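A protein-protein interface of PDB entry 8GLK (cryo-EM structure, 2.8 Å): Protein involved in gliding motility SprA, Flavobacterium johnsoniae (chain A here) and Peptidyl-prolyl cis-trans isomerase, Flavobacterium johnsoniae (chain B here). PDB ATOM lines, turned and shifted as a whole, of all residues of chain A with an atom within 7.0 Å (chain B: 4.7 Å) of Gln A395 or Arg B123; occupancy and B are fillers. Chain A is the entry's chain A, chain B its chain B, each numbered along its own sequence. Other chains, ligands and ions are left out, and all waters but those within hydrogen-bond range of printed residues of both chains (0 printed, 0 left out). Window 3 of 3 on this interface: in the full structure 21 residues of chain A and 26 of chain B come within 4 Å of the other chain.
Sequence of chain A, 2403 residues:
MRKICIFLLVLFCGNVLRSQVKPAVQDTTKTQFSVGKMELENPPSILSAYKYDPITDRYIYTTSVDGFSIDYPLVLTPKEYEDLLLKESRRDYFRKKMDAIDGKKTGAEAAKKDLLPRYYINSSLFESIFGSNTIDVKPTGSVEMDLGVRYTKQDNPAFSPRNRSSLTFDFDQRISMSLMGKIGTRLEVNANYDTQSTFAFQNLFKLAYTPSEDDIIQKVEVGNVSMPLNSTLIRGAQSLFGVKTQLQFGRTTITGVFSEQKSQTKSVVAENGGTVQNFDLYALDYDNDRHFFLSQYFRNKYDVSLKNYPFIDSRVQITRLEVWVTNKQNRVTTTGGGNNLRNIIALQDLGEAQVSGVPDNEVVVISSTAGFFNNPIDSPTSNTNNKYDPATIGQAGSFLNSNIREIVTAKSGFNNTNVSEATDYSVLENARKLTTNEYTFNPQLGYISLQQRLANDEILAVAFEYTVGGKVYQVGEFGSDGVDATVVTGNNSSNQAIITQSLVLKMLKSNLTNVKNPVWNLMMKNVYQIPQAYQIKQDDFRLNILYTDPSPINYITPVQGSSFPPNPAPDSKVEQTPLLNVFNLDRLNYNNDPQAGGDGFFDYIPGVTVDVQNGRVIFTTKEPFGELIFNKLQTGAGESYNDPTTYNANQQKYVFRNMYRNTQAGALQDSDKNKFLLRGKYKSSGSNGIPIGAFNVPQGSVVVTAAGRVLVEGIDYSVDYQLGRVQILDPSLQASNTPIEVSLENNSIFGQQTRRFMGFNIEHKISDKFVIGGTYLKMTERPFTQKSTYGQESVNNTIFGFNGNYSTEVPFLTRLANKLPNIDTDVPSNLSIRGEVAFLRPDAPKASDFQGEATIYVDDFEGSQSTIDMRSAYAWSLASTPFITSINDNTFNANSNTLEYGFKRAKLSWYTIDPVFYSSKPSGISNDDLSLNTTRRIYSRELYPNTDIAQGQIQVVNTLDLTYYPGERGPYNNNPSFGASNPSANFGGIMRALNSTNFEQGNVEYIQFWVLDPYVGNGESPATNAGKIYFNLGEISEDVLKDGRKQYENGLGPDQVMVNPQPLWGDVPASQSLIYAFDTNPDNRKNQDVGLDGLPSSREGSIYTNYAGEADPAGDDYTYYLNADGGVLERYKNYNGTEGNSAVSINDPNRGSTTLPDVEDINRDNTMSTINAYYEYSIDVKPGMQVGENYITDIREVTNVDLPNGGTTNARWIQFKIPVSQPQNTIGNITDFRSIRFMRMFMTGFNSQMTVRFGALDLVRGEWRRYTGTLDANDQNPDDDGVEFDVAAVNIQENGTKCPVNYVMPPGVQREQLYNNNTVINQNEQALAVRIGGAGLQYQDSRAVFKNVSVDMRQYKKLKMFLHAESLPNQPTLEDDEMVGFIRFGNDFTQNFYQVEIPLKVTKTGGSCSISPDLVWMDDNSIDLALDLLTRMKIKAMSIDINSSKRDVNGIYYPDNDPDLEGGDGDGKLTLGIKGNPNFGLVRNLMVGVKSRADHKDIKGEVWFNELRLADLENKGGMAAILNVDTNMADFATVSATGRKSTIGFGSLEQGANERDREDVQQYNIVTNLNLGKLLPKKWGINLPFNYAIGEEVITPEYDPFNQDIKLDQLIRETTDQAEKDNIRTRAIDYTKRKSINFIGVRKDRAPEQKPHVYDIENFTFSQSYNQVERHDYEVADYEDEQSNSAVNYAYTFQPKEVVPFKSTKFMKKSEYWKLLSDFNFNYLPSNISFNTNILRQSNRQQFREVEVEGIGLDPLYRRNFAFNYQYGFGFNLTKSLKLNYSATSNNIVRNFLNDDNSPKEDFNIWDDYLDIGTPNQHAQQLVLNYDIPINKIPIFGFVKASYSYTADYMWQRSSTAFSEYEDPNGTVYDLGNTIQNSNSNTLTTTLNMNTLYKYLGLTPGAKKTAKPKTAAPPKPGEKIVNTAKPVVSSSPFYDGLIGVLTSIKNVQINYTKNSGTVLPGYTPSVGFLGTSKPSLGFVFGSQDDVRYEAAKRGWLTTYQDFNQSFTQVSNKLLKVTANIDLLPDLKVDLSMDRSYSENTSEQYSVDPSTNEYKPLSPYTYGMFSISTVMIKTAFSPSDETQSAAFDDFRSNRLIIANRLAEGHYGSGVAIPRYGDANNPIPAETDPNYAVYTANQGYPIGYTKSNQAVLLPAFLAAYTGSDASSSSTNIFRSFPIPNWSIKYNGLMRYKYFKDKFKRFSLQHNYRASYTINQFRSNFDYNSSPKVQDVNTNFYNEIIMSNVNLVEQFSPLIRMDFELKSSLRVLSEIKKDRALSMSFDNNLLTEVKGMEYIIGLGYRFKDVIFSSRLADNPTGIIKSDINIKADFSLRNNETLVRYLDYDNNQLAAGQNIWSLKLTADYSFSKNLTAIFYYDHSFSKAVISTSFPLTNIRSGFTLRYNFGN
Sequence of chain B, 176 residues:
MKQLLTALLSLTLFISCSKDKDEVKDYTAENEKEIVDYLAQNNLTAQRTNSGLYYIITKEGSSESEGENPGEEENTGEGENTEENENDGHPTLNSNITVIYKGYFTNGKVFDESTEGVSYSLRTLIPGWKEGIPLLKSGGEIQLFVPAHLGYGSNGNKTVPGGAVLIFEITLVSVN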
ATOM      1  N   ALA A 391       7.311   0.530   4.472  1.00  0.00           N
ATOM      2  CA  ALA A 391       6.520   0.193   3.295  1.00  0.00           C
ATOM      3  C   ALA A 391       7.106   0.803   2.028  1.00  0.00           C
ATOM      4  O   ALA A 391       7.002   0.208   0.950  1.00  0.00           O
ATOM      5  CB  ALA A 391       5.075   0.649   3.482  1.00  0.00           C
ATOM      6  N   THR A 392       7.719   1.977   2.135  1.00  0.00           N
ATOM      7  CA  THR A 392       8.270   2.697   0.993  1.00  0.00           C
ATOM      8  C   THR A 392       9.793   2.616   0.955  1.00  0.00           C
ATOM      9  O   THR A 392      10.469   3.585   0.615  1.00  0.00           O
ATOM     10  CB  THR A 392       7.826   4.157   1.007  1.00  0.00           C
ATOM     11  OG1 THR A 392       8.574   4.877   1.996  1.00  0.00           O
ATOM     12  CG2 THR A 392       6.344   4.263   1.324  1.00  0.00           C
ATOM     13  N   ILE A 393      10.351   1.457   1.301  1.00  0.00           N
ATOM     14  CA  ILE A 393      11.803   1.304   1.360  1.00  0.00           C
ATOM     15  C   ILE A 393      12.358   1.414  -0.058  1.00  0.00           C
ATOM     16  O   ILE A 393      12.159   0.524  -0.890  1.00  0.00           O
ATOM     17  CB  ILE A 393      12.202  -0.021   2.020  1.00  0.00           C
ATOM     18  CG1 ILE A 393      12.079   0.089   3.540  1.00  0.00           C
ATOM     19  CG2 ILE A 393      13.628  -0.397   1.660  1.00  0.00           C
ATOM     20  CD1 ILE A 393      12.460  -1.172   4.278  1.00  0.00           C
ATOM     21  N   GLY A 394      13.037   2.522  -0.339  1.00  0.00           N
ATOM     22  CA  GLY A 394      13.693   2.713  -1.624  1.00  0.00           C
ATOM     23  C   GLY A 394      12.761   2.774  -2.814  1.00  0.00           C
ATOM     24  O   GLY A 394      13.090   2.241  -3.881  1.00  0.00           O
ATOM     25  N   GLN A 395      11.598   3.411  -2.662  1.00  0.00           N
ATOM     26  CA  GLN A 395      10.645   3.461  -3.770  1.00  0.00           C
ATOM     27  C   GLN A 395      10.989   4.575  -4.755  1.00  0.00           C
ATOM     28  O   GLN A 395      11.351   4.310  -5.906  1.00  0.00           O
ATOM     29  CB  GLN A 395       9.223   3.639  -3.226  1.00  0.00           C
ATOM     30  CG  GLN A 395       8.631   2.390  -2.599  1.00  0.00           C
ATOM     31  CD  GLN A 395       7.957   1.490  -3.614  1.00  0.00           C
ATOM     32  OE1 GLN A 395       8.597   0.980  -4.533  1.00  0.00           O
ATOM     33  NE2 GLN A 395       6.653   1.291  -3.452  1.00  0.00           N
ATOM     34  N   ALA A 396      10.881   5.826  -4.323  1.00  0.00           N
ATOM     35  CA  ALA A 396      11.249   6.942  -5.188  1.00  0.00           C
ATOM     36  C   ALA A 396      12.149   7.964  -4.514  1.00  0.00           C
ATOM     37  O   ALA A 396      13.070   8.481  -5.153  1.00  0.00           O
ATOM     38  CB  ALA A 396       9.981   7.636  -5.711  1.00  0.00           C
ATOM     39  N   GLY A 397      11.908   8.270  -3.242  1.00  0.00           N
ATOM     40  CA  GLY A 397      12.670   9.284  -2.543  1.00  0.00           C
ATOM     41  C   GLY A 397      12.883   8.942  -1.085  1.00  0.00           C
ATOM     42  O   GLY A 397      13.053   9.831  -0.246  1.00  0.00           O
ATOM     43  N   SER A 398      12.865   7.651  -0.776  1.00  0.00           N
ATOM     44  CA  SER A 398      13.003   7.203   0.599  1.00  0.00           C
ATOM     45  C   SER A 398      14.418   7.442   1.110  1.00  0.00           C
ATOM     46  O   SER A 398      15.356   7.691   0.348  1.00  0.00           O
ATOM     47  CB  SER A 398      12.659   5.720   0.715  1.00  0.00           C
ATOM     48  OG  SER A 398      12.712   5.289   2.063  1.00  0.00           O
ATOM     49  N   LEU A 400      15.854   5.028   2.867  1.00  0.00           N
ATOM     50  CA  LEU A 400      16.291   3.667   3.139  1.00  0.00           C
ATOM     51  C   LEU A 400      16.451   2.896   1.838  1.00  0.00           C
ATOM     52  O   LEU A 400      15.701   3.111   0.882  1.00  0.00           O
ATOM     53  CB  LEU A 400      15.295   2.938   4.050  1.00  0.00           C
ATOM     54  CG  LEU A 400      15.041   3.548   5.428  1.00  0.00           C
ATOM     55  CD1 LEU A 400      13.993   2.745   6.178  1.00  0.00           C
ATOM     56  CD2 LEU A 400      16.328   3.630   6.225  1.00  0.00           C
ATOM     57  N   ASP A2127      15.749  -5.454  -8.747  1.00  0.00           N
ATOM     58  CA  ASP A2127      14.416  -5.395  -8.166  1.00  0.00           C
ATOM     59  C   ASP A2127      14.407  -6.114  -6.820  1.00  0.00           C
ATOM     60  O   ASP A2127      14.929  -7.233  -6.717  1.00  0.00           O
ATOM     61  CB  ASP A2127      13.404  -6.037  -9.117  1.00  0.00           C
ATOM     62  CG  ASP A2127      12.017  -5.424  -9.011  1.00  0.00           C
ATOM     63  OD1 ASP A2127      11.840  -4.449  -8.254  1.00  0.00           O
ATOM     64  OD2 ASP A2127      11.097  -5.924  -9.691  1.00  0.00           O
ATOM     65  N   PRO A2128      13.842  -5.512  -5.768  1.00  0.00           N
ATOM     66  CA  PRO A2128      13.788  -6.202  -4.468  1.00  0.00           C
ATOM     67  C   PRO A2128      13.010  -7.505  -4.495  1.00  0.00           C
ATOM     68  O   PRO A2128      13.236  -8.359  -3.629  1.00  0.00           O
ATOM     69  CB  PRO A2128      13.116  -5.169  -3.549  1.00  0.00           C
ATOM     70  CG  PRO A2128      12.475  -4.174  -4.479  1.00  0.00           C
ATOM     71  CD  PRO A2128      13.389  -4.118  -5.657  1.00  0.00           C
ATOM     72  N   ASN A2129      12.104  -7.688  -5.451  1.00  0.00           N
ATOM     73  CA  ASN A2129      11.307  -8.902  -5.547  1.00  0.00           C
ATOM     74  C   ASN A2129      11.984  -9.991  -6.368  1.00  0.00           C
ATOM     75  O   ASN A2129      11.366 -11.029  -6.622  1.00  0.00           O
ATOM     76  CB  ASN A2129       9.932  -8.583  -6.140  1.00  0.00           C
ATOM     77  CG  ASN A2129       8.956  -8.069  -5.101  1.00  0.00           C
ATOM     78  OD1 ASN A2129       9.334  -7.782  -3.967  1.00  0.00           O
ATOM     79  ND2 ASN A2129       7.691  -7.950  -5.486  1.00  0.00           N
ATOM     80  N   TYR A2133      10.659 -13.712  -6.186  1.00  0.00           N
ATOM     81  CA  TYR A2133      10.139 -14.336  -7.397  1.00  0.00           C
ATOM     82  C   TYR A2133      10.936 -15.581  -7.765  1.00  0.00           C
ATOM     83  O   TYR A2133      10.370 -16.566  -8.252  1.00  0.00           O
ATOM     84  CB  TYR A2133      10.150 -13.331  -8.548  1.00  0.00           C
ATOM     85  CG  TYR A2133       8.854 -12.568  -8.703  1.00  0.00           C
ATOM     86  CD1 TYR A2133       8.395 -11.732  -7.695  1.00  0.00           C
ATOM     87  CD2 TYR A2133       8.094 -12.678  -9.859  1.00  0.00           C
ATOM     88  CE1 TYR A2133       7.214 -11.032  -7.830  1.00  0.00           C
ATOM     89  CE2 TYR A2133       6.911 -11.980 -10.004  1.00  0.00           C
ATOM     90  CZ  TYR A2133       6.476 -11.159  -8.987  1.00  0.00           C
ATOM     91  OH  TYR A2133       5.298 -10.463  -9.127  1.00  0.00           O
ATOM     92  N   ILE A2141       0.605 -16.435  -7.572  1.00  0.00           N
ATOM     93  CA  ILE A2141       1.101 -15.104  -7.222  1.00  0.00           C
ATOM     94  C   ILE A2141       0.807 -14.777  -5.764  1.00  0.00           C
ATOM     95  O   ILE A2141       1.682 -14.311  -5.025  1.00  0.00           O
ATOM     96  CB  ILE A2141       0.505 -14.046  -8.167  1.00  0.00           C
ATOM     97  CG1 ILE A2141       0.920 -14.336  -9.607  1.00  0.00           C
ATOM     98  CG2 ILE A2141       0.940 -12.652  -7.752  1.00  0.00           C
ATOM     99  CD1 ILE A2141       2.412 -14.291  -9.812  1.00  0.00           C
ATOM    100  N   VAL A2227      -4.136  -5.829  -1.707  1.00  0.00           N
ATOM    101  CA  VAL A2227      -4.416  -7.210  -1.332  1.00  0.00           C
ATOM    102  C   VAL A2227      -3.163  -8.016  -1.032  1.00  0.00           C
ATOM    103  O   VAL A2227      -3.279  -9.128  -0.496  1.00  0.00           O
ATOM    104  CB  VAL A2227      -5.252  -7.927  -2.415  1.00  0.00           C
ATOM    105  CG1 VAL A2227      -6.652  -7.343  -2.478  1.00  0.00           C
ATOM    106  CG2 VAL A2227      -4.565  -7.829  -3.767  1.00  0.00           C
ATOM    107  N   GLN A2228      -1.975  -7.508  -1.348  1.00  0.00           N
ATOM    108  CA  GLN A2228      -0.734  -8.240  -1.150  1.00  0.00           C
ATOM    109  C   GLN A2228       0.184  -7.477  -0.206  1.00  0.00           C
ATOM    110  O   GLN A2228       0.192  -6.243  -0.183  1.00  0.00           O
ATOM    111  CB  GLN A2228      -0.022  -8.496  -2.483  1.00  0.00           C
ATOM    112  CG  GLN A2228      -0.704  -9.539  -3.352  1.00  0.00           C
ATOM    113  CD  GLN A2228      -0.096  -9.637  -4.737  1.00  0.00           C
ATOM    114  OE1 GLN A2228       0.914  -8.998  -5.031  1.00  0.00           O
ATOM    115  NE2 GLN A2228      -0.708 -10.444  -5.595  1.00  0.00           N
ATOM    116  N   ASP A2229       0.949  -8.223   0.586  1.00  0.00           N
ATOM    117  CA  ASP A2229       1.877  -7.630   1.536  1.00  0.00           C
ATOM    118  C   ASP A2229       3.257  -7.481   0.894  1.00  0.00           C
ATOM    119  O   ASP A2229       3.428  -7.652  -0.316  1.00  0.00           O
ATOM    120  CB  ASP A2229       1.922  -8.456   2.821  1.00  0.00           C
ATOM    121  CG  ASP A2229       2.198  -9.927   2.570  1.00  0.00           C
ATOM    122  OD1 ASP A2229       3.197 -10.249   1.896  1.00  0.00           O
ATOM    123  OD2 ASP A2229       1.415 -10.765   3.060  1.00  0.00           O
ATOM    124  N   VAL A2230       4.261  -7.151   1.712  1.00  0.00           N
ATOM    125  CA  VAL A2230       5.616  -6.945   1.215  1.00  0.00           C
ATOM    126  C   VAL A2230       6.202  -8.220   0.623  1.00  0.00           C
ATOM    127  O   VAL A2230       7.072  -8.153  -0.252  1.00  0.00           O
ATOM    128  CB  VAL A2230       6.503  -6.384   2.351  1.00  0.00           C
ATOM    129  CG1 VAL A2230       6.635  -7.394   3.484  1.00  0.00           C
ATOM    130  CG2 VAL A2230       7.871  -5.969   1.822  1.00  0.00           C
ATOM    131  N   THR A2232       4.526 -10.273  -1.219  1.00  0.00           N
ATOM    132  CA  THR A2232       3.620 -10.595  -2.322  1.00  0.00           C
ATOM    133  C   THR A2232       2.590 -11.651  -1.935  1.00  0.00           C
ATOM    134  O   THR A2232       2.002 -12.297  -2.807  1.00  0.00           O
ATOM    135  CB  THR A2232       4.384 -11.037  -3.578  1.00  0.00           C
ATOM    136  OG1 THR A2232       4.921 -12.351  -3.379  1.00  0.00           O
ATOM    137  CG2 THR A2232       5.517 -10.070  -3.889  1.00  0.00           C
ATOM    138  N   LEU B  93       5.251  -1.370 -12.895  1.00  0.00           N
ATOM    139  CA  LEU B  93       4.951  -2.307 -11.816  1.00  0.00           C
ATOM    140  C   LEU B  93       5.647  -1.911 -10.520  1.00  0.00           C
ATOM    141  O   LEU B  93       5.188  -2.277  -9.432  1.00  0.00           O
ATOM    142  CB  LEU B  93       5.348  -3.724 -12.243  1.00  0.00           C
ATOM    143  CG  LEU B  93       4.925  -4.922 -11.390  1.00  0.00           C
ATOM    144  CD1 LEU B  93       4.658  -6.118 -12.282  1.00  0.00           C
ATOM    145  CD2 LEU B  93       5.995  -5.276 -10.371  1.00  0.00           C
ATOM    146  N   ASN B  94       6.739  -1.156 -10.613  1.00  0.00           N
ATOM    147  CA  ASN B  94       7.468  -0.658  -9.448  1.00  0.00           C
ATOM    148  C   ASN B  94       7.350   0.863  -9.447  1.00  0.00           C
ATOM    149  O   ASN B  94       8.219   1.577  -9.951  1.00  0.00           O
ATOM    150  CB  ASN B  94       8.929  -1.115  -9.492  1.00  0.00           C
ATOM    151  CG  ASN B  94       9.079  -2.610  -9.295  1.00  0.00           C
ATOM    152  OD1 ASN B  94       8.423  -3.205  -8.442  1.00  0.00           O
ATOM    153  ND2 ASN B  94       9.943  -3.226 -10.093  1.00  0.00           N
ATOM    154  N   ASN B  96       5.109   4.081  -6.975  1.00  0.00           N
ATOM    155  CA  ASN B  96       4.118   4.490  -5.988  1.00  0.00           C
ATOM    156  C   ASN B  96       3.197   5.540  -6.595  1.00  0.00           C
ATOM    157  O   ASN B  96       3.666   6.538  -7.153  1.00  0.00           O
ATOM    158  CB  ASN B  96       4.801   5.038  -4.735  1.00  0.00           C
ATOM    159  CG  ASN B  96       3.831   5.256  -3.592  1.00  0.00           C
ATOM    160  OD1 ASN B  96       3.184   6.298  -3.502  1.00  0.00           O
ATOM    161  ND2 ASN B  96       3.731   4.272  -2.706  1.00  0.00           N
ATOM    162  N   SER B 121       1.365   1.023  -3.767  1.00  0.00           N
ATOM    163  CA  SER B 121       2.574   0.574  -4.450  1.00  0.00           C
ATOM    164  C   SER B 121       2.309   0.076  -5.865  1.00  0.00           C
ATOM    165  O   SER B 121       3.265  -0.114  -6.624  1.00  0.00           O
ATOM    166  CB  SER B 121       3.254  -0.532  -3.639  1.00  0.00           C
ATOM    167  OG  SER B 121       4.448  -0.964  -4.269  1.00  0.00           O
ATOM    168  N   LEU B 122       1.044  -0.180  -6.210  1.00  0.00           N
ATOM    169  CA  LEU B 122       0.596  -0.600  -7.538  1.00  0.00           C
ATOM    170  C   LEU B 122       1.000  -2.046  -7.814  1.00  0.00           C
ATOM    171  O   LEU B 122       0.526  -2.658  -8.776  1.00  0.00           O
ATOM    172  CB  LEU B 122       1.134   0.354  -8.618  1.00  0.00           C
ATOM    173  CG  LEU B 122       0.694   0.275 -10.086  1.00  0.00           C
ATOM    174  CD1 LEU B 122       0.834   1.645 -10.721  1.00  0.00           C
ATOM    175  CD2 LEU B 122       1.493  -0.734 -10.895  1.00  0.00           C
ATOM    176  N   ARG B 123       1.822  -2.624  -6.941  1.00  0.00           N
ATOM    177  CA  ARG B 123       2.147  -4.041  -7.007  1.00  0.00           C
ATOM    178  C   ARG B 123       1.432  -4.848  -5.934  1.00  0.00           C
ATOM    179  O   ARG B 123       1.389  -6.079  -6.027  1.00  0.00           O
ATOM    180  CB  ARG B 123       3.660  -4.254  -6.876  1.00  0.00           C
ATOM    181  CG  ARG B 123       4.183  -4.105  -5.457  1.00  0.00           C
ATOM    182  CD  ARG B 123       5.616  -4.599  -5.336  1.00  0.00           C
ATOM    183  NE  ARG B 123       6.552  -3.766  -6.081  1.00  0.00           N
ATOM    184  CZ  ARG B 123       7.332  -2.846  -5.531  1.00  0.00           C
ATOM    185  NH1 ARG B 123       7.317  -2.615  -4.229  1.00  0.00           N
ATOM    186  NH2 ARG B 123       8.151  -2.141  -6.307  1.00  0.00           N
ATOM    187  N   THR B 124       0.881  -4.182  -4.923  1.00  0.00           N
ATOM    188  CA  THR B 124       0.120  -4.821  -3.862  1.00  0.00           C
ATOM    189  C   THR B 124      -1.381  -4.788  -4.114  1.00  0.00           C
ATOM    190  O   THR B 124      -2.146  -5.287  -3.284  1.00  0.00           O
ATOM    191  CB  THR B 124       0.434  -4.152  -2.521  1.00  0.00           C
ATOM    192  OG1 THR B 124      -0.110  -2.826  -2.509  1.00  0.00           O
ATOM    193  CG2 THR B 124       1.936  -4.077  -2.305  1.00  0.00           C
ATOM    194  N   LEU B 125      -1.815  -4.218  -5.234  1.00  0.00           N
ATOM    195  CA  LEU B 125      -3.227  -4.031  -5.517  1.00  0.00           C
ATOM    196  C   LEU B 125      -3.782  -5.220  -6.297  1.00  0.00           C
ATOM    197  O   LEU B 125      -3.070  -6.169  -6.630  1.00  0.00           O
ATOM    198  CB  LEU B 125      -3.440  -2.725  -6.281  1.00  0.00           C
ATOM    199  CG  LEU B 125      -2.725  -1.506  -5.698  1.00  0.00           C
ATOM    200  CD1 LEU B 125      -2.905  -0.296  -6.593  1.00  0.00           C
ATOM    201  CD2 LEU B 125      -3.230  -1.214  -4.297  1.00  0.00           C
ATOM    202  N   LYS B 130      -3.669  -3.262 -11.629  1.00  0.00           N
ATOM    203  CA  LYS B 130      -2.372  -3.459 -12.269  1.00  0.00           C
ATOM    204  C   LYS B 130      -2.464  -3.353 -13.784  1.00  0.00           C
ATOM    205  O   LYS B 130      -1.482  -2.987 -14.438  1.00  0.00           O
ATOM    206  CB  LYS B 130      -1.790  -4.816 -11.876  1.00  0.00           C
ATOM    207  CG  LYS B 130      -1.415  -4.941 -10.415  1.00  0.00           C
ATOM    208  CD  LYS B 130      -0.817  -6.305 -10.134  1.00  0.00           C
ATOM    209  CE  LYS B 130      -0.410  -6.439  -8.681  1.00  0.00           C
ATOM    210  NZ  LYS B 130       0.195  -7.767  -8.399  1.00  0.00           N
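Among the printed residues, pairs that only touch across the chains: Gln A395 with Arg B123 (3.6 Å), Asn A2129 with Arg B123 (3.9 Å), Val A2227 with Leu B125 (3.6 Å) and Gln A2228 with Lys B130 (3.7 Å).
O of Thr B124 lies within hydrogen-bond range of N of Val A2227, at 2.6 Å. N of Gln A2228 lies within hydrogen-bond range of O of Thr B124 (3.0 Å). The side-chain hydroxyl (OG) of Ser B121 lies within hydrogen-bond range of the side-chain amide nitrogen (NE2) of Gln A395 (3.3 Å). The side-chain amide oxygen of Gln A2228 sits close to the backbone carbonyl oxygen of Arg B123, 3.1 Å away. The side-chain carboxylate of Asp A2127 lies within hydrogen-bond range of the side-chain amide nitrogen of Asn B94 (2.9 Å).
Of the 19 printed residues of chain A, 5 touch a printed residue of chain B. Printed residues of chain A that touch a printed residue of chain B: Gln A395, Asp A2127, Asn A2129, Val A2227 and Gln A2228. Hydrophobic or aromatic side chains of chain A within 4 Å of the printed part of chain B: Val A2227. Printed residues of chain B that touch a printed residue of chain A: Asn B94, Ser B121, Arg B123, Thr B124, Leu B125 and Lys B130. Along chain B the printed residues that touch a printed residue of chain A span positions 94 to 130. Among the printed residues, no Asp or Glu carboxylate lies within 4 Å of a Lys or Arg side-chain nitrogen of the other chain.
Gln A395 touches just these residues of chain B: Ser B121 (3.3 Å) and Arg B123 (3.6 Å). Arg B123 touches just these residues of chain A: Gln A395, Asn A2129 and Gln A2228. Printed residues of chain A within 4 Å of Ser B121: Gln A395. Printed residues of chain A within 4 Å of Leu B125: Val A2227 (3.6 Å). Printed residues of chain A within 4 Å of Lys B130: Gln A2228 (3.7 Å). Of the printed residues of chain B, Gln A2228 touches Arg B123 (3.1 Å), Thr B124 (3.0 Å) and Lys B130 (3.7 Å). Ala A396 touches none of the printed residues of chain B. Ala A391 touches none of the printed residues of chain B. The nearest residue of chain B that does not touch Gln A395 is Asn B96 (4.2 Å).
The guanidinium group (NH2) of Arg B123 sits at hydrogen-bond distance from the side-chain amide oxygen (OD1) of Asn B94. OG of Ser B121 lies within hydrogen-bond range of NH1 of Arg B123 (3.3 Å). The backbone carbonyl oxygen of Arg B123 sits at hydrogen-bond distance from the side-chain amino group of Lys B130.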
